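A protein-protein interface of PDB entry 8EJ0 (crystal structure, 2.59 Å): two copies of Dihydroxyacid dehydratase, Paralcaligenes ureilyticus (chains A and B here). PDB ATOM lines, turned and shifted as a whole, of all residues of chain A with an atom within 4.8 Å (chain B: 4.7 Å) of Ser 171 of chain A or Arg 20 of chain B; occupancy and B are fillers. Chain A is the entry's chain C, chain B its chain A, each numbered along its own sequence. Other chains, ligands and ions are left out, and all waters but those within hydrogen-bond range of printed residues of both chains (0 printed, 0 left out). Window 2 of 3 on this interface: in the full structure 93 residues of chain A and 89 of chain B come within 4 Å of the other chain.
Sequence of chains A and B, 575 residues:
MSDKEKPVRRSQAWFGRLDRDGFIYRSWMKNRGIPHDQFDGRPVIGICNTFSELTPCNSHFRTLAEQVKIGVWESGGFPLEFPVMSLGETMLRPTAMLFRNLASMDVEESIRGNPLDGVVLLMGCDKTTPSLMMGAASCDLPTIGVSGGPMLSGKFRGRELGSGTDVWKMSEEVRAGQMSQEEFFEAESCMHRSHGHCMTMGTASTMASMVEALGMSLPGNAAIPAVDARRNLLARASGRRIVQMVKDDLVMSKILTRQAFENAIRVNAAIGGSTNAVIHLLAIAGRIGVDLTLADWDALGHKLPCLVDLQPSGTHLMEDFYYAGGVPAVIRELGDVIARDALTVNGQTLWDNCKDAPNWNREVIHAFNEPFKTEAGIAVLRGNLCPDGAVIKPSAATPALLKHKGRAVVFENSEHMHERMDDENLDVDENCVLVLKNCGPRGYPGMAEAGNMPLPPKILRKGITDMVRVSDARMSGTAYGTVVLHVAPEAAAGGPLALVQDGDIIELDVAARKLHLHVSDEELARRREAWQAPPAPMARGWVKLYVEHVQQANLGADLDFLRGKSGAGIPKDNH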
ATOM      1  N   ASP A 166     -14.692  15.874 -25.600  1.00  0.00           N
ATOM      2  CA  ASP A 166     -13.820  15.366 -26.650  1.00  0.00           C
ATOM      3  C   ASP A 166     -12.587  16.231 -26.873  1.00  0.00           C
ATOM      4  O   ASP A 166     -11.668  15.794 -27.574  1.00  0.00           O
ATOM      5  CB  ASP A 166     -14.600  15.218 -27.959  1.00  0.00           C
ATOM      6  CG  ASP A 166     -15.461  13.970 -27.978  1.00  0.00           C
ATOM      7  OD1 ASP A 166     -15.036  12.948 -27.396  1.00  0.00           O
ATOM      8  OD2 ASP A 166     -16.561  14.009 -28.567  1.00  0.00           O
ATOM      9  N   VAL A 167     -12.539  17.437 -26.303  1.00  0.00           N
ATOM     10  CA  VAL A 167     -11.297  18.204 -26.326  1.00  0.00           C
ATOM     11  C   VAL A 167     -10.258  17.539 -25.433  1.00  0.00           C
ATOM     12  O   VAL A 167      -9.109  17.335 -25.838  1.00  0.00           O
ATOM     13  CB  VAL A 167     -11.545  19.664 -25.909  1.00  0.00           C
ATOM     14  CG1 VAL A 167     -10.224  20.417 -25.824  1.00  0.00           C
ATOM     15  CG2 VAL A 167     -12.474  20.344 -26.889  1.00  0.00           C
ATOM     16  N   TRP A 168     -10.649  17.183 -24.206  1.00  0.00           N
ATOM     17  CA  TRP A 168      -9.729  16.477 -23.320  1.00  0.00           C
ATOM     18  C   TRP A 168      -9.392  15.096 -23.867  1.00  0.00           C
ATOM     19  O   TRP A 168      -8.241  14.653 -23.784  1.00  0.00           O
ATOM     20  CB  TRP A 168     -10.320  16.348 -21.913  1.00  0.00           C
ATOM     21  CG  TRP A 168     -11.227  17.466 -21.491  1.00  0.00           C
ATOM     22  CD1 TRP A 168     -12.536  17.359 -21.119  1.00  0.00           C
ATOM     23  CD2 TRP A 168     -10.893  18.857 -21.384  1.00  0.00           C
ATOM     24  NE1 TRP A 168     -13.039  18.595 -20.792  1.00  0.00           N
ATOM     25  CE2 TRP A 168     -12.051  19.531 -20.946  1.00  0.00           C
ATOM     26  CE3 TRP A 168      -9.729  19.597 -21.617  1.00  0.00           C
ATOM     27  CZ2 TRP A 168     -12.079  20.908 -20.740  1.00  0.00           C
ATOM     28  CZ3 TRP A 168      -9.761  20.965 -21.410  1.00  0.00           C
ATOM     29  CH2 TRP A 168     -10.927  21.606 -20.975  1.00  0.00           C
ATOM     30  N   LYS A 169     -10.382  14.404 -24.434  1.00  0.00           N
ATOM     31  CA  LYS A 169     -10.168  13.029 -24.879  1.00  0.00           C
ATOM     32  C   LYS A 169      -9.248  12.977 -26.091  1.00  0.00           C
ATOM     33  O   LYS A 169      -8.283  12.204 -26.116  1.00  0.00           O
ATOM     34  CB  LYS A 169     -11.508  12.365 -25.191  1.00  0.00           C
ATOM     35  CG  LYS A 169     -11.414  10.864 -25.404  1.00  0.00           C
ATOM     36  CD  LYS A 169     -12.205  10.427 -26.624  1.00  0.00           C
ATOM     37  CE  LYS A 169     -12.199   8.915 -26.771  1.00  0.00           C
ATOM     38  NZ  LYS A 169     -12.886   8.479 -28.016  1.00  0.00           N
ATOM     39  N   MET A 170      -9.532  13.790 -27.112  1.00  0.00           N
ATOM     40  CA  MET A 170      -8.697  13.776 -28.308  1.00  0.00           C
ATOM     41  C   MET A 170      -7.317  14.365 -28.039  1.00  0.00           C
ATOM     42  O   MET A 170      -6.337  13.940 -28.661  1.00  0.00           O
ATOM     43  CB  MET A 170      -9.388  14.527 -29.447  1.00  0.00           C
ATOM     44  CG  MET A 170     -10.628  13.833 -29.988  1.00  0.00           C
ATOM     45  SD  MET A 170     -11.275  14.615 -31.480  1.00  0.00           S
ATOM     46  CE  MET A 170     -11.710  16.236 -30.857  1.00  0.00           C
ATOM     47  N   SER A 171      -7.217  15.333 -27.125  1.00  0.00           N
ATOM     48  CA  SER A 171      -5.911  15.894 -26.786  1.00  0.00           C
ATOM     49  C   SER A 171      -5.011  14.838 -26.157  1.00  0.00           C
ATOM     50  O   SER A 171      -3.860  14.662 -26.570  1.00  0.00           O
ATOM     51  CB  SER A 171      -6.072  17.089 -25.845  1.00  0.00           C
ATOM     52  OG  SER A 171      -4.813  17.600 -25.444  1.00  0.00           O
ATOM     53  N   GLU A 172      -5.527  14.118 -25.156  1.00  0.00           N
ATOM     54  CA  GLU A 172      -4.736  13.079 -24.503  1.00  0.00           C
ATOM     55  C   GLU A 172      -4.323  11.987 -25.478  1.00  0.00           C
ATOM     56  O   GLU A 172      -3.259  11.380 -25.314  1.00  0.00           O
ATOM     57  CB  GLU A 172      -5.521  12.481 -23.335  1.00  0.00           C
ATOM     58  CG  GLU A 172      -5.741  13.443 -22.179  1.00  0.00           C
ATOM     59  CD  GLU A 172      -4.461  13.759 -21.432  1.00  0.00           C
ATOM     60  OE1 GLU A 172      -4.094  12.984 -20.523  1.00  0.00           O
ATOM     61  OE2 GLU A 172      -3.817  14.778 -21.759  1.00  0.00           O
ATOM     62  N   GLU A 173      -5.142  11.723 -26.499  1.00  0.00           N
ATOM     63  CA  GLU A 173      -4.785  10.706 -27.482  1.00  0.00           C
ATOM     64  C   GLU A 173      -3.682  11.189 -28.416  1.00  0.00           C
ATOM     65  O   GLU A 173      -2.890  10.376 -28.908  1.00  0.00           O
ATOM     66  CB  GLU A 173      -6.020  10.290 -28.280  1.00  0.00           C
ATOM     67  CG  GLU A 173      -7.062   9.557 -27.450  1.00  0.00           C
ATOM     68  CD  GLU A 173      -8.301   9.203 -28.245  1.00  0.00           C
ATOM     69  OE1 GLU A 173      -8.265   9.313 -29.489  1.00  0.00           O
ATOM     70  OE2 GLU A 173      -9.314   8.816 -27.625  1.00  0.00           O
ATOM     71  N   VAL A 174      -3.613  12.497 -28.676  1.00  0.00           N
ATOM     72  CA  VAL A 174      -2.514  13.032 -29.474  1.00  0.00           C
ATOM     73  C   VAL A 174      -1.198  12.901 -28.719  1.00  0.00           C
ATOM     74  O   VAL A 174      -0.171  12.521 -29.293  1.00  0.00           O
ATOM     75  CB  VAL A 174      -2.800  14.494 -29.868  1.00  0.00           C
ATOM     76  CG1 VAL A 174      -1.592  15.103 -30.562  1.00  0.00           C
ATOM     77  CG2 VAL A 174      -4.023  14.575 -30.767  1.00  0.00           C
ATOM     78  N   ARG A 175      -1.209  13.203 -27.419  1.00  0.00           N
ATOM     79  CA  ARG A 175      -0.002  13.094 -26.610  1.00  0.00           C
ATOM     80  C   ARG A 175       0.370  11.645 -26.323  1.00  0.00           C
ATOM     81  O   ARG A 175       1.541  11.364 -26.041  1.00  0.00           O
ATOM     82  CB  ARG A 175      -0.187  13.868 -25.303  1.00  0.00           C
ATOM     83  CG  ARG A 175      -0.981  15.154 -25.484  1.00  0.00           C
ATOM     84  CD  ARG A 175      -1.061  15.993 -24.220  1.00  0.00           C
ATOM     85  NE  ARG A 175      -1.140  15.183 -23.008  1.00  0.00           N
ATOM     86  CZ  ARG A 175      -0.214  15.188 -22.055  1.00  0.00           C
ATOM     87  NH1 ARG A 175       0.851  15.967 -22.171  1.00  0.00           N
ATOM     88  NH2 ARG A 175      -0.358  14.424 -20.983  1.00  0.00           N
ATOM     89  N   PHE A 184      -6.806  16.099 -35.063  1.00  0.00           N
ATOM     90  CA  PHE A 184      -7.352  16.808 -33.910  1.00  0.00           C
ATOM     91  C   PHE A 184      -7.760  18.231 -34.272  1.00  0.00           C
ATOM     92  O   PHE A 184      -8.764  18.744 -33.764  1.00  0.00           O
ATOM     93  CB  PHE A 184      -6.330  16.813 -32.773  1.00  0.00           C
ATOM     94  CG  PHE A 184      -6.734  17.656 -31.596  1.00  0.00           C
ATOM     95  CD1 PHE A 184      -7.782  17.272 -30.779  1.00  0.00           C
ATOM     96  CD2 PHE A 184      -6.056  18.828 -31.300  1.00  0.00           C
ATOM     97  CE1 PHE A 184      -8.156  18.043 -29.693  1.00  0.00           C
ATOM     98  CE2 PHE A 184      -6.423  19.603 -30.216  1.00  0.00           C
ATOM     99  CZ  PHE A 184      -7.474  19.210 -29.411  1.00  0.00           C
ATOM    100  N   PRO A 454      -3.702  17.021 -17.521  1.00  0.00           N
ATOM    101  CA  PRO A 454      -3.332  15.867 -18.345  1.00  0.00           C
ATOM    102  C   PRO A 454      -2.351  14.952 -17.631  1.00  0.00           C
ATOM    103  O   PRO A 454      -1.606  15.367 -16.742  1.00  0.00           O
ATOM    104  CB  PRO A 454      -2.695  16.506 -19.586  1.00  0.00           C
ATOM    105  CG  PRO A 454      -2.225  17.848 -19.118  1.00  0.00           C
ATOM    106  CD  PRO A 454      -3.236  18.293 -18.104  1.00  0.00           C
ATOM    107  N   ASP B  19      -1.915  23.820 -30.182  1.00  0.00           N
ATOM    108  CA  ASP B  19      -2.016  22.755 -29.190  1.00  0.00           C
ATOM    109  C   ASP B  19      -3.481  22.637 -28.785  1.00  0.00           C
ATOM    110  O   ASP B  19      -4.385  23.064 -29.510  1.00  0.00           O
ATOM    111  CB  ASP B  19      -1.065  23.034 -28.015  1.00  0.00           C
ATOM    112  CG  ASP B  19      -1.359  24.351 -27.321  1.00  0.00           C
ATOM    113  OD1 ASP B  19      -1.059  24.469 -26.115  1.00  0.00           O
ATOM    114  OD2 ASP B  19      -1.908  25.261 -27.979  1.00  0.00           O
ATOM    115  N   ARG B  20      -3.729  22.043 -27.614  1.00  0.00           N
ATOM    116  CA  ARG B  20      -5.103  21.859 -27.152  1.00  0.00           C
ATOM    117  C   ARG B  20      -5.804  23.195 -26.946  1.00  0.00           C
ATOM    118  O   ARG B  20      -6.997  23.330 -27.238  1.00  0.00           O
ATOM    119  CB  ARG B  20      -5.117  21.048 -25.857  1.00  0.00           C
ATOM    120  CG  ARG B  20      -6.503  20.858 -25.262  1.00  0.00           C
ATOM    121  CD  ARG B  20      -6.427  20.499 -23.787  1.00  0.00           C
ATOM    122  NE  ARG B  20      -5.818  21.568 -23.001  1.00  0.00           N
ATOM    123  CZ  ARG B  20      -5.651  21.527 -21.683  1.00  0.00           C
ATOM    124  NH1 ARG B  20      -6.051  20.467 -20.995  1.00  0.00           N
ATOM    125  NH2 ARG B  20      -5.086  22.547 -21.052  1.00  0.00           N
ATOM    126  N   ASP B  21      -5.077  24.196 -26.446  1.00  0.00           N
ATOM    127  CA  ASP B  21      -5.692  25.493 -26.182  1.00  0.00           C
ATOM    128  C   ASP B  21      -6.112  26.192 -27.469  1.00  0.00           C
ATOM    129  O   ASP B  21      -7.133  26.888 -27.486  1.00  0.00           O
ATOM    130  CB  ASP B  21      -4.737  26.374 -25.379  1.00  0.00           C
ATOM    131  CG  ASP B  21      -4.455  25.816 -23.998  1.00  0.00           C
ATOM    132  OD1 ASP B  21      -5.239  24.962 -23.531  1.00  0.00           O
ATOM    133  OD2 ASP B  21      -3.456  26.234 -23.376  1.00  0.00           O
ATOM    134  N   GLY B  22      -5.346  26.022 -28.550  1.00  0.00           N
ATOM    135  CA  GLY B  22      -5.753  26.591 -29.825  1.00  0.00           C
ATOM    136  C   GLY B  22      -7.076  26.034 -30.313  1.00  0.00           C
ATOM    137  O   GLY B  22      -7.867  26.742 -30.941  1.00  0.00           O
ATOM    138  N   PHE B  23      -7.333  24.755 -30.031  1.00  0.00           N
ATOM    139  CA  PHE B  23      -8.637  24.174 -30.325  1.00  0.00           C
ATOM    140  C   PHE B  23      -9.734  24.888 -29.545  1.00  0.00           C
ATOM    141  O   PHE B  23     -10.779  25.242 -30.101  1.00  0.00           O
ATOM    142  CB  PHE B  23      -8.624  22.678 -29.996  1.00  0.00           C
ATOM    143  CG  PHE B  23      -9.810  21.919 -30.528  1.00  0.00           C
ATOM    144  CD1 PHE B  23     -11.039  21.981 -29.890  1.00  0.00           C
ATOM    145  CD2 PHE B  23      -9.690  21.124 -31.656  1.00  0.00           C
ATOM    146  CE1 PHE B  23     -12.126  21.281 -30.378  1.00  0.00           C
ATOM    147  CE2 PHE B  23     -10.774  20.418 -32.145  1.00  0.00           C
ATOM    148  CZ  PHE B  23     -11.992  20.498 -31.505  1.00  0.00           C
ATOM    149  N   ILE B  24      -9.503  25.116 -28.251  1.00  0.00           N
ATOM    150  CA  ILE B  24     -10.513  25.746 -27.404  1.00  0.00           C
ATOM    151  C   ILE B  24     -10.799  27.167 -27.874  1.00  0.00           C
ATOM    152  O   ILE B  24     -11.960  27.587 -27.957  1.00  0.00           O
ATOM    153  CB  ILE B  24     -10.060  25.720 -25.932  1.00  0.00           C
ATOM    154  CG1 ILE B  24      -9.809  24.283 -25.473  1.00  0.00           C
ATOM    155  CG2 ILE B  24     -11.088  26.399 -25.041  1.00  0.00           C
ATOM    156  CD1 ILE B  24      -9.274  24.182 -24.062  1.00  0.00           C
ATOM    157  N   HIS B 575      -7.424  26.909 -19.039  1.00  0.00           N
ATOM    158  CA  HIS B 575      -7.658  25.487 -18.803  1.00  0.00           C
ATOM    159  C   HIS B 575      -6.349  24.743 -18.560  1.00  0.00           C
ATOM    160  O   HIS B 575      -5.267  25.276 -18.801  1.00  0.00           O
ATOM    161  CB  HIS B 575      -8.408  24.862 -19.983  1.00  0.00           C
ATOM    162  CG  HIS B 575      -9.791  25.402 -20.178  1.00  0.00           C
ATOM    163  ND1 HIS B 575     -10.043  26.587 -20.835  1.00  0.00           N
ATOM    164  CD2 HIS B 575     -10.998  24.920 -19.796  1.00  0.00           C
ATOM    165  CE1 HIS B 575     -11.344  26.811 -20.851  1.00  0.00           C
ATOM    166  NE2 HIS B 575     -11.947  25.815 -20.228  1.00  0.00           N
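The guanidinium group (NH2) of Arg 20 of chain B lies within salt-bridge range of the side-chain carboxylate (OD1) of Asp 21 of chain B.
Val 167 of chain A touches Arg 20 of chain B.
Phe 23 of chain B touches Val 167 of chain A.
Val 167 of chain A touches Ile 24 of chain B.
Trp 168 of chain A touches Arg 20 of chain B.
Trp 168 of chain A touches His 575 of chain B (CH2 to CD2, 3.5 Å).
Arg 20 of chain B touches Ser 171 of chain A.
CE2 of Phe 23 of chain B touches O of Phe 184 of chain A, at 3.1 Å.
Printed residues of chain B within 4 Å of Val 167 of chain A: Arg 20 (3.8 Å), Phe 23 (3.6 Å) and Ile 24 (3.9 Å).
Of the printed residues of chain B, Trp 168 of chain A touches Arg 20 and His 575.
Ser 171 of chain A touches just one residue of chain B: Arg 20.
Of the printed residues of chain B, Phe 184 of chain A touches Phe 23 (3.1 Å).
Of the printed residues of chain A, Phe 23 of chain B touches Val 167 (3.6 Å) and Phe 184 (3.1 Å).
Of the printed residues of chain A, Ile 24 of chain B touches Val 167.
The nearest residue of chain A that does not touch Arg 20 of chain B is Phe 184 of chain A (4.03 Å).
Of the 7 printed residues of chain B, 4 touch a printed residue of chain A.
Hydrophobic or aromatic side chains of chain B within 4 Å of the printed part of chain A: Phe 23, Ile 24 and His 575.
Of the 12 printed residues of chain A, 4 touch a printed residue of chain B.
Hydrophobic or aromatic side chains of chain A that line the printed part of chain B: Val 167, Trp 168 and Phe 184.
No position is printed for both chains.
Of the 7 pairs that touch across the chains among the printed residues, none has its exchanged pair printed and touching as well.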
